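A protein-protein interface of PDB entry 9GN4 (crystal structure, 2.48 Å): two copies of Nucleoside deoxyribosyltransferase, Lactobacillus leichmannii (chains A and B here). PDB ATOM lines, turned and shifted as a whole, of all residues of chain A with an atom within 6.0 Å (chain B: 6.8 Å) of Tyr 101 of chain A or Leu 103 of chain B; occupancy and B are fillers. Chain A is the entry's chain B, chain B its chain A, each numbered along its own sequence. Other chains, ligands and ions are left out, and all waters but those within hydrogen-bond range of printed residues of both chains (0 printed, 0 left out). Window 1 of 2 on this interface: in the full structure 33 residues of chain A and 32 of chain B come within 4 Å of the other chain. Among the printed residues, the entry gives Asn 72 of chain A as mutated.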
ATOM      1  N   TYR A  69      -3.497   2.030   3.805  1.00  0.00           N
ATOM      2  CA  TYR A  69      -2.696   3.219   4.074  1.00  0.00           C
ATOM      3  C   TYR A  69      -2.596   3.403   5.585  1.00  0.00           C
ATOM      4  O   TYR A  69      -1.513   3.544   6.147  1.00  0.00           O
ATOM      5  CB  TYR A  69      -3.265   4.448   3.351  1.00  0.00           C
ATOM      6  CG  TYR A  69      -2.647   5.782   3.761  1.00  0.00           C
ATOM      7  CD1 TYR A  69      -1.403   6.186   3.291  1.00  0.00           C
ATOM      8  CD2 TYR A  69      -3.336   6.660   4.582  1.00  0.00           C
ATOM      9  CE1 TYR A  69      -0.842   7.393   3.682  1.00  0.00           C
ATOM     10  CE2 TYR A  69      -2.785   7.858   4.998  1.00  0.00           C
ATOM     11  CZ  TYR A  69      -1.537   8.232   4.542  1.00  0.00           C
ATOM     12  OH  TYR A  69      -1.058   9.436   4.975  1.00  0.00           O
ATOM     13  N   ASN A  72      -0.385   0.912   7.509  1.00  0.00           N
ATOM     14  CA  ASN A  72       1.022   1.267   7.411  1.00  0.00           C
ATOM     15  C   ASN A  72       1.402   2.380   8.395  1.00  0.00           C
ATOM     16  O   ASN A  72       2.376   2.252   9.124  1.00  0.00           O
ATOM     17  CB  ASN A  72       1.373   1.631   5.977  1.00  0.00           C
ATOM     18  CG  ASN A  72       1.485   0.419   5.085  1.00  0.00           C
ATOM     19  OD1 ASN A  72       1.484   0.550   3.864  1.00  0.00           O
ATOM     20  ND2 ASN A  72       1.535  -0.765   5.658  1.00  0.00           N
ATOM     21  N   LEU A  73       0.609   3.455   8.452  1.00  0.00           N
ATOM     22  CA  LEU A  73       0.893   4.543   9.374  1.00  0.00           C
ATOM     23  C   LEU A  73       0.855   4.007  10.793  1.00  0.00           C
ATOM     24  O   LEU A  73       1.694   4.361  11.614  1.00  0.00           O
ATOM     25  CB  LEU A  73      -0.093   5.700   9.248  1.00  0.00           C
ATOM     26  CG  LEU A  73      -0.143   6.418   7.899  1.00  0.00           C
ATOM     27  CD1 LEU A  73      -0.923   7.724   8.084  1.00  0.00           C
ATOM     28  CD2 LEU A  73       1.212   6.705   7.307  1.00  0.00           C
ATOM     29  N   ASN A  74      -0.129   3.159  11.071  1.00  0.00           N
ATOM     30  CA  ASN A  74      -0.294   2.567  12.389  1.00  0.00           C
ATOM     31  C   ASN A  74       0.919   1.713  12.756  1.00  0.00           C
ATOM     32  O   ASN A  74       1.394   1.741  13.900  1.00  0.00           O
ATOM     33  CB  ASN A  74      -1.583   1.756  12.435  1.00  0.00           C
ATOM     34  CG  ASN A  74      -1.851   1.224  13.816  1.00  0.00           C
ATOM     35  OD1 ASN A  74      -1.804   0.014  14.033  1.00  0.00           O
ATOM     36  ND2 ASN A  74      -2.088   2.108  14.765  1.00  0.00           N
ATOM     37  N   ILE A  76       3.939   2.142  11.613  1.00  0.00           N
ATOM     38  CA  ILE A  76       5.061   3.015  11.937  1.00  0.00           C
ATOM     39  C   ILE A  76       4.928   3.601  13.349  1.00  0.00           C
ATOM     40  O   ILE A  76       5.873   3.564  14.137  1.00  0.00           O
ATOM     41  CB  ILE A  76       5.222   4.108  10.882  1.00  0.00           C
ATOM     42  CG1 ILE A  76       5.600   3.494   9.568  1.00  0.00           C
ATOM     43  CG2 ILE A  76       6.234   5.162  11.333  1.00  0.00           C
ATOM     44  CD1 ILE A  76       5.442   4.410   8.380  1.00  0.00           C
ATOM     45  N   LYS A  77       3.751   4.156  13.660  1.00  0.00           N
ATOM     46  CA  LYS A  77       3.577   4.939  14.879  1.00  0.00           C
ATOM     47  C   LYS A  77       3.603   4.055  16.130  1.00  0.00           C
ATOM     48  O   LYS A  77       4.100   4.504  17.155  1.00  0.00           O
ATOM     49  CB  LYS A  77       2.340   5.839  14.871  1.00  0.00           C
ATOM     50  CG  LYS A  77       1.036   5.171  15.222  1.00  0.00           C
ATOM     51  CD  LYS A  77      -0.170   6.110  15.080  1.00  0.00           C
ATOM     52  CE  LYS A  77      -1.394   5.396  15.578  1.00  0.00           C
ATOM     53  NZ  LYS A  77      -2.643   6.035  15.200  1.00  0.00           N
ATOM     54  N   GLY A  96       9.715   6.947   0.863  1.00  0.00           N
ATOM     55  CA  GLY A  96      10.003   8.339   1.181  1.00  0.00           C
ATOM     56  C   GLY A  96       8.941   8.923   2.113  1.00  0.00           C
ATOM     57  O   GLY A  96       9.277   9.462   3.154  1.00  0.00           O
ATOM     58  N   MET A  97       7.665   8.740   1.761  1.00  0.00           N
ATOM     59  CA  MET A  97       6.562   9.281   2.534  1.00  0.00           C
ATOM     60  C   MET A  97       6.638   8.743   3.956  1.00  0.00           C
ATOM     61  O   MET A  97       6.578   9.490   4.949  1.00  0.00           O
ATOM     62  CB  MET A  97       5.228   8.928   1.874  1.00  0.00           C
ATOM     63  CG  MET A  97       4.027   9.480   2.606  1.00  0.00           C
ATOM     64  SD  MET A  97       3.512   8.351   3.915  1.00  0.00           S
ATOM     65  CE  MET A  97       2.583   9.493   4.938  1.00  0.00           C
ATOM     66  N   GLU A  98       6.873   7.442   4.043  1.00  0.00           N
ATOM     67  CA  GLU A  98       6.938   6.766   5.330  1.00  0.00           C
ATOM     68  C   GLU A  98       8.080   7.289   6.208  1.00  0.00           C
ATOM     69  O   GLU A  98       7.929   7.366   7.442  1.00  0.00           O
ATOM     70  CB  GLU A  98       7.044   5.259   5.104  1.00  0.00           C
ATOM     71  CG  GLU A  98       5.751   4.684   4.533  1.00  0.00           C
ATOM     72  CD  GLU A  98       5.813   3.229   4.111  1.00  0.00           C
ATOM     73  OE1 GLU A  98       4.724   2.582   4.066  1.00  0.00           O
ATOM     74  OE2 GLU A  98       6.950   2.794   3.784  1.00  0.00           O
ATOM     75  N   LEU A  99       9.232   7.594   5.586  1.00  0.00           N
ATOM     76  CA  LEU A  99      10.361   8.177   6.303  1.00  0.00           C
ATOM     77  C   LEU A  99       9.927   9.512   6.918  1.00  0.00           C
ATOM     78  O   LEU A  99      10.142   9.779   8.087  1.00  0.00           O
ATOM     79  CB  LEU A  99      11.574   8.360   5.392  1.00  0.00           C
ATOM     80  CG  LEU A  99      12.125   7.089   4.739  1.00  0.00           C
ATOM     81  CD1 LEU A  99      13.277   7.366   3.821  1.00  0.00           C
ATOM     82  CD2 LEU A  99      12.578   6.098   5.794  1.00  0.00           C
ATOM     83  N   GLY A 100       9.263  10.349   6.131  1.00  0.00           N
ATOM     84  CA  GLY A 100       8.807  11.630   6.638  1.00  0.00           C
ATOM     85  C   GLY A 100       7.764  11.470   7.745  1.00  0.00           C
ATOM     86  O   GLY A 100       7.807  12.188   8.729  1.00  0.00           O
ATOM     87  N   TYR A 101       6.843  10.517   7.603  1.00  0.00           N
ATOM     88  CA  TYR A 101       5.922  10.211   8.682  1.00  0.00           C
ATOM     89  C   TYR A 101       6.667   9.776   9.949  1.00  0.00           C
ATOM     90  O   TYR A 101       6.448  10.330  11.024  1.00  0.00           O
ATOM     91  CB  TYR A 101       4.884   9.204   8.169  1.00  0.00           C
ATOM     92  CG  TYR A 101       3.823   8.928   9.209  1.00  0.00           C
ATOM     93  CD1 TYR A 101       2.830   9.867   9.485  1.00  0.00           C
ATOM     94  CD2 TYR A 101       3.836   7.742   9.923  1.00  0.00           C
ATOM     95  CE1 TYR A 101       1.866   9.611  10.437  1.00  0.00           C
ATOM     96  CE2 TYR A 101       2.880   7.479  10.885  1.00  0.00           C
ATOM     97  CZ  TYR A 101       1.896   8.414  11.139  1.00  0.00           C
ATOM     98  OH  TYR A 101       0.991   8.143  12.117  1.00  0.00           O
ATOM     99  N   ALA A 102       7.603   8.855   9.809  1.00  0.00           N
ATOM    100  CA  ALA A 102       8.348   8.337  10.947  1.00  0.00           C
ATOM    101  C   ALA A 102       9.079   9.442  11.697  1.00  0.00           C
ATOM    102  O   ALA A 102       9.103   9.452  12.948  1.00  0.00           O
ATOM    103  CB  ALA A 102       9.351   7.309  10.461  1.00  0.00           C
ATOM    104  N   LEU A 103       9.695  10.339  10.921  1.00  0.00           N
ATOM    105  CA  LEU A 103      10.363  11.510  11.481  1.00  0.00           C
ATOM    106  C   LEU A 103       9.375  12.278  12.350  1.00  0.00           C
ATOM    107  O   LEU A 103       9.635  12.518  13.522  1.00  0.00           O
ATOM    108  CB  LEU A 103      10.921  12.439  10.408  1.00  0.00           C
ATOM    109  CG  LEU A 103      11.549  13.740  10.936  1.00  0.00           C
ATOM    110  CD1 LEU A 103      12.966  13.536  11.489  1.00  0.00           C
ATOM    111  CD2 LEU A 103      11.526  14.804   9.850  1.00  0.00           C
ATOM    112  N   SER A 104       8.206  12.587  11.791  1.00  0.00           N
ATOM    113  CA  SER A 104       7.224  13.360  12.526  1.00  0.00           C
ATOM    114  C   SER A 104       6.784  12.604  13.781  1.00  0.00           C
ATOM    115  O   SER A 104       6.337  13.224  14.737  1.00  0.00           O
ATOM    116  CB  SER A 104       6.014  13.705  11.649  1.00  0.00           C
ATOM    117  OG  SER A 104       5.117  12.603  11.474  1.00  0.00           O
ATOM    118  N   GLN A 105       6.848  11.266  13.776  1.00  0.00           N
ATOM    119  CA  GLN A 105       6.365  10.507  14.916  1.00  0.00           C
ATOM    120  C   GLN A 105       7.469  10.294  15.950  1.00  0.00           C
ATOM    121  O   GLN A 105       7.274   9.547  16.889  1.00  0.00           O
ATOM    122  CB  GLN A 105       5.772   9.177  14.470  1.00  0.00           C
ATOM    123  CG  GLN A 105       4.460   9.319  13.710  1.00  0.00           C
ATOM    124  CD  GLN A 105       3.370  10.017  14.504  1.00  0.00           C
ATOM    125  OE1 GLN A 105       3.057   9.718  15.656  1.00  0.00           O
ATOM    126  NE2 GLN A 105       2.786  11.016  13.895  1.00  0.00           N
ATOM    127  N   GLY A 106       8.629  10.928  15.766  1.00  0.00           N
ATOM    128  CA  GLY A 106       9.686  10.890  16.758  1.00  0.00           C
ATOM    129  C   GLY A 106      10.479   9.578  16.770  1.00  0.00           C
ATOM    130  O   GLY A 106      11.159   9.317  17.747  1.00  0.00           O
ATOM    131  N   ILE B  76       8.968  24.423   3.426  1.00  0.00           N
ATOM    132  CA  ILE B  76       7.659  23.808   3.608  1.00  0.00           C
ATOM    133  C   ILE B  76       6.936  24.438   4.795  1.00  0.00           C
ATOM    134  O   ILE B  76       5.765  24.798   4.689  1.00  0.00           O
ATOM    135  CB  ILE B  76       7.772  22.291   3.760  1.00  0.00           C
ATOM    136  CG1 ILE B  76       8.275  21.646   2.488  1.00  0.00           C
ATOM    137  CG2 ILE B  76       6.457  21.683   4.221  1.00  0.00           C
ATOM    138  CD1 ILE B  76       8.804  20.241   2.705  1.00  0.00           C
ATOM    139  N   MET B  82       1.462  22.961   0.350  1.00  0.00           N
ATOM    140  CA  MET B  82       2.448  22.048  -0.190  1.00  0.00           C
ATOM    141  C   MET B  82       1.949  21.540  -1.534  1.00  0.00           C
ATOM    142  O   MET B  82       0.882  20.930  -1.612  1.00  0.00           O
ATOM    143  CB  MET B  82       2.603  20.843   0.745  1.00  0.00           C
ATOM    144  CG  MET B  82       3.535  19.803   0.231  1.00  0.00           C
ATOM    145  SD  MET B  82       5.238  20.396   0.147  1.00  0.00           S
ATOM    146  CE  MET B  82       5.863  19.073  -0.910  1.00  0.00           C
ATOM    147  N   GLY B  96       8.332  12.544  -2.007  1.00  0.00           N
ATOM    148  CA  GLY B  96       7.594  11.718  -1.075  1.00  0.00           C
ATOM    149  C   GLY B  96       7.903  12.118   0.364  1.00  0.00           C
ATOM    150  O   GLY B  96       6.984  12.318   1.153  1.00  0.00           O
ATOM    151  N   MET B  97       9.197  12.272   0.687  1.00  0.00           N
ATOM    152  CA  MET B  97       9.604  12.602   2.036  1.00  0.00           C
ATOM    153  C   MET B  97       8.941  13.916   2.430  1.00  0.00           C
ATOM    154  O   MET B  97       8.357  14.048   3.516  1.00  0.00           O
ATOM    155  CB  MET B  97      11.129  12.662   2.141  1.00  0.00           C
ATOM    156  CG  MET B  97      11.684  13.166   3.474  1.00  0.00           C
ATOM    157  SD  MET B  97      11.636  14.961   3.565  1.00  0.00           S
ATOM    158  CE  MET B  97      11.715  15.150   5.348  1.00  0.00           C
ATOM    159  N   GLU B  98       8.989  14.861   1.506  1.00  0.00           N
ATOM    160  CA  GLU B  98       8.446  16.194   1.728  1.00  0.00           C
ATOM    161  C   GLU B  98       6.936  16.168   1.953  1.00  0.00           C
ATOM    162  O   GLU B  98       6.429  16.995   2.711  1.00  0.00           O
ATOM    163  CB  GLU B  98       8.823  17.101   0.560  1.00  0.00           C
ATOM    164  CG  GLU B  98      10.311  17.407   0.534  1.00  0.00           C
ATOM    165  CD  GLU B  98      10.764  18.183  -0.689  1.00  0.00           C
ATOM    166  OE1 GLU B  98      11.842  18.829  -0.595  1.00  0.00           O
ATOM    167  OE2 GLU B  98      10.053  18.116  -1.723  1.00  0.00           O
ATOM    168  N   LEU B  99       6.223  15.256   1.274  1.00  0.00           N
ATOM    169  CA  LEU B  99       4.786  15.094   1.475  1.00  0.00           C
ATOM    170  C   LEU B  99       4.537  14.722   2.933  1.00  0.00           C
ATOM    171  O   LEU B  99       3.683  15.316   3.604  1.00  0.00           O
ATOM    172  CB  LEU B  99       4.159  14.100   0.501  1.00  0.00           C
ATOM    173  CG  LEU B  99       4.340  14.413  -0.994  1.00  0.00           C
ATOM    174  CD1 LEU B  99       3.741  13.322  -1.857  1.00  0.00           C
ATOM    175  CD2 LEU B  99       3.736  15.756  -1.393  1.00  0.00           C
ATOM    176  N   GLY B 100       5.334  13.770   3.427  1.00  0.00           N
ATOM    177  CA  GLY B 100       5.260  13.357   4.820  1.00  0.00           C
ATOM    178  C   GLY B 100       5.576  14.499   5.776  1.00  0.00           C
ATOM    179  O   GLY B 100       4.906  14.682   6.783  1.00  0.00           O
ATOM    180  N   TYR B 101       6.606  15.281   5.467  1.00  0.00           N
ATOM    181  CA  TYR B 101       6.962  16.409   6.319  1.00  0.00           C
ATOM    182  C   TYR B 101       5.814  17.426   6.343  1.00  0.00           C
ATOM    183  O   TYR B 101       5.367  17.846   7.416  1.00  0.00           O
ATOM    184  CB  TYR B 101       8.311  16.986   5.886  1.00  0.00           C
ATOM    185  CG  TYR B 101       8.760  18.125   6.791  1.00  0.00           C
ATOM    186  CD1 TYR B 101       9.268  17.887   8.057  1.00  0.00           C
ATOM    187  CD2 TYR B 101       8.660  19.442   6.364  1.00  0.00           C
ATOM    188  CE1 TYR B 101       9.626  18.927   8.896  1.00  0.00           C
ATOM    189  CE2 TYR B 101       9.045  20.491   7.178  1.00  0.00           C
ATOM    190  CZ  TYR B 101       9.533  20.236   8.448  1.00  0.00           C
ATOM    191  OH  TYR B 101       9.846  21.309   9.231  1.00  0.00           O
ATOM    192  N   ALA B 102       5.280  17.753   5.162  1.00  0.00           N
ATOM    193  CA  ALA B 102       4.190  18.701   5.049  1.00  0.00           C
ATOM    194  C   ALA B 102       2.979  18.281   5.881  1.00  0.00           C
ATOM    195  O   ALA B 102       2.336  19.127   6.522  1.00  0.00           O
ATOM    196  CB  ALA B 102       3.795  18.839   3.603  1.00  0.00           C
ATOM    197  N   LEU B 103       2.649  16.989   5.819  1.00  0.00           N
ATOM    198  CA  LEU B 103       1.590  16.429   6.633  1.00  0.00           C
ATOM    199  C   LEU B 103       1.871  16.738   8.108  1.00  0.00           C
ATOM    200  O   LEU B 103       1.040  17.300   8.798  1.00  0.00           O
ATOM    201  CB  LEU B 103       1.445  14.931   6.421  1.00  0.00           C
ATOM    202  CG  LEU B 103       0.461  14.219   7.367  1.00  0.00           C
ATOM    203  CD1 LEU B 103      -1.002  14.399   6.919  1.00  0.00           C
ATOM    204  CD2 LEU B 103       0.841  12.732   7.527  1.00  0.00           C
ATOM    205  N   SER B 104       3.097  16.483   8.549  1.00  0.00           N
ATOM    206  CA  SER B 104       3.495  16.784   9.946  1.00  0.00           C
ATOM    207  C   SER B 104       3.326  18.270  10.271  1.00  0.00           C
ATOM    208  O   SER B 104       3.109  18.585  11.444  1.00  0.00           O
ATOM    209  CB  SER B 104       4.910  16.393  10.169  1.00  0.00           C
ATOM    210  OG  SER B 104       5.798  17.462   9.882  1.00  0.00           O
ATOM    211  N   GLN B 105       3.453  19.140   9.278  1.00  0.00           N
ATOM    212  CA  GLN B 105       3.404  20.596   9.548  1.00  0.00           C
ATOM    213  C   GLN B 105       1.977  21.117   9.353  1.00  0.00           C
ATOM    214  O   GLN B 105       1.793  22.341   9.391  1.00  0.00           O
ATOM    215  CB  GLN B 105       4.430  21.282   8.653  1.00  0.00           C
ATOM    216  CG  GLN B 105       5.867  20.853   8.919  1.00  0.00           C
ATOM    217  CD  GLN B 105       6.278  21.051  10.359  1.00  0.00           C
ATOM    218  OE1 GLN B 105       6.246  22.166  10.888  1.00  0.00           O
ATOM    219  NE2 GLN B 105       6.666  19.966  11.010  1.00  0.00           N
ATOM    220  N   GLY B 106       1.015  20.218   9.155  1.00  0.00           N
ATOM    221  CA  GLY B 106      -0.364  20.653   9.044  1.00  0.00           C
ATOM    222  C   GLY B 106      -0.711  21.409   7.761  1.00  0.00           C
ATOM    223  O   GLY B 106      -1.701  22.113   7.761  1.00  0.00           O
ATOM    224  N   LYS B 107       0.032  21.187   6.671  1.00  0.00           N
ATOM    225  CA  LYS B 107      -0.188  21.887   5.410  1.00  0.00           C
ATOM    226  C   LYS B 107      -1.122  21.089   4.512  1.00  0.00           C
ATOM    227  O   LYS B 107      -1.056  19.863   4.482  1.00  0.00           O
ATOM    228  CB  LYS B 107       1.104  22.038   4.598  1.00  0.00           C
ATOM    229  CG  LYS B 107       2.272  22.665   5.340  1.00  0.00           C
ATOM    230  CD  LYS B 107       1.945  24.074   5.816  1.00  0.00           C
ATOM    231  CE  LYS B 107       3.045  24.585   6.674  1.00  0.00           C
ATOM    232  NZ  LYS B 107       2.829  25.967   7.070  1.00  0.00           N
ATOM    233  N   VAL B 109      -1.931  19.372   1.193  1.00  0.00           N
ATOM    234  CA  VAL B 109      -1.033  18.657   0.312  1.00  0.00           C
ATOM    235  C   VAL B 109      -1.772  18.391  -1.000  1.00  0.00           C
ATOM    236  O   VAL B 109      -2.644  17.529  -1.047  1.00  0.00           O
ATOM    237  CB  VAL B 109      -0.518  17.347   0.946  1.00  0.00           C
ATOM    238  CG1 VAL B 109       0.346  16.574  -0.042  1.00  0.00           C
ATOM    239  CG2 VAL B 109       0.247  17.584   2.245  1.00  0.00           C
ATOM    240  N   GLY B 128      -2.568   8.467  -0.096  1.00  0.00           N
ATOM    241  CA  GLY B 128      -3.040   8.718   1.260  1.00  0.00           C
ATOM    242  C   GLY B 128      -2.565  10.057   1.848  1.00  0.00           C
ATOM    243  O   GLY B 128      -3.354  10.752   2.494  1.00  0.00           O
ATOM    244  N   VAL B 129      -1.277  10.420   1.705  1.00  0.00           N
ATOM    245  CA  VAL B 129      -0.821  11.677   2.293  1.00  0.00           C
ATOM    246  C   VAL B 129      -1.559  12.833   1.631  1.00  0.00           C
ATOM    247  O   VAL B 129      -1.620  13.910   2.187  1.00  0.00           O
ATOM    248  CB  VAL B 129       0.645  12.140   2.160  1.00  0.00           C
ATOM    249  CG1 VAL B 129       1.413  12.183   3.456  1.00  0.00           C
ATOM    250  CG2 VAL B 129       1.378  11.576   0.958  1.00  0.00           C
ATOM    251  N   ASP B 131      -4.117  15.388   0.293  1.00  0.00           N
ATOM    252  CA  ASP B 131      -5.463  15.872   0.574  1.00  0.00           C
ATOM    253  C   ASP B 131      -6.302  15.916  -0.696  1.00  0.00           C
ATOM    254  O   ASP B 131      -7.523  15.892  -0.606  1.00  0.00           O
ATOM    255  CB  ASP B 131      -5.389  17.231   1.258  1.00  0.00           C
ATOM    256  CG  ASP B 131      -4.762  17.158   2.648  1.00  0.00           C
ATOM    257  OD1 ASP B 131      -5.236  16.302   3.426  1.00  0.00           O
ATOM    258  OD2 ASP B 131      -3.787  17.921   2.922  1.00  0.00           O
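N of Val 129 of chain B is in hydrogen-bond range of OH of Tyr 69 of chain A (3.4 Å).
The backbone carbonyl oxygen (O) of Tyr 101 of chain B sits at hydrogen-bond distance from the side-chain hydroxyl (OG) of Ser 104 of chain B (2.5 Å). The side-chain hydroxyl of Ser 104 of chain B is in hydrogen-bond range of the side-chain amide nitrogen of Gln 105 of chain B. O of Tyr 101 of chain A sits at hydrogen-bond distance from OG of Ser 104 of chain A (2.7 Å).
Tyr 69 of chain A touches Gly 128 of chain B. Gly 96 of chain B touches Gly 96 of chain A. Gly 96 of chain A touches Met 97 of chain B. Met 97 of chain A touches Gly 96 of chain B. N of Met 97 of chain A touches N of Met 97 of chain B, at 3.997 Å. CE of Met 97 of chain A touches CG1 of Val 129 of chain B (3.3 Å). O of Met 97 of chain B touches CA of Gly 100 of chain A (3.97 Å). Tyr 101 of chain A touches Leu 103 of chain B. CB of Ser 104 of chain A touches CB of Ser 104 of chain B, 3.3 Å away.
Asn 74 of chain A touches none of the printed residues of chain B. Printed residues of chain B within 4 Å of Gly 96 of chain A: Gly 96 (3.8 Å) and Met 97 (3.3 Å). Of the printed residues of chain B, Met 97 of chain A touches Gly 96, Met 97 and Val 129. Of the printed residues of chain B, Tyr 101 of chain A touches Leu 103. Printed residues of chain A within 4 Å of Gly 96 of chain B: Gly 96 (3.8 Å) and Met 97 (3.4 Å). Printed residues of chain A within 4 Å of Leu 103 of chain B: Tyr 101 (3.9998 Å). The nearest printed residue of chain A that does not touch Ser 104 of chain B is Gly 100 of chain A (5.3 Å).
Hydrophobic or aromatic side chains of chain A within 4 Å of the printed part of chain B: Tyr 69, Met 97 and Tyr 101. Among the printed residues, 10 pairs touch across the chains.
Met 97 of chain A touches its own counterpart, Met 97 of chain B. Gly 100 of chain A touches Met 97 of chain B, but with the chains exchanged Met 97 of chain A does not touch Gly 100 of chain B (4.1 Å). Tyr 101 of chain A touches Leu 103 of chain B, but with the chains exchanged Leu 103 of chain A does not touch Tyr 101 of chain B (4.2 Å). Ser 104 of chain B touches its own counterpart, Ser 104 of chain A. Positions printed for both chains: 76, 96, 97, 98, 99, 100, 101, 102, 103, 104, 105 and 106.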
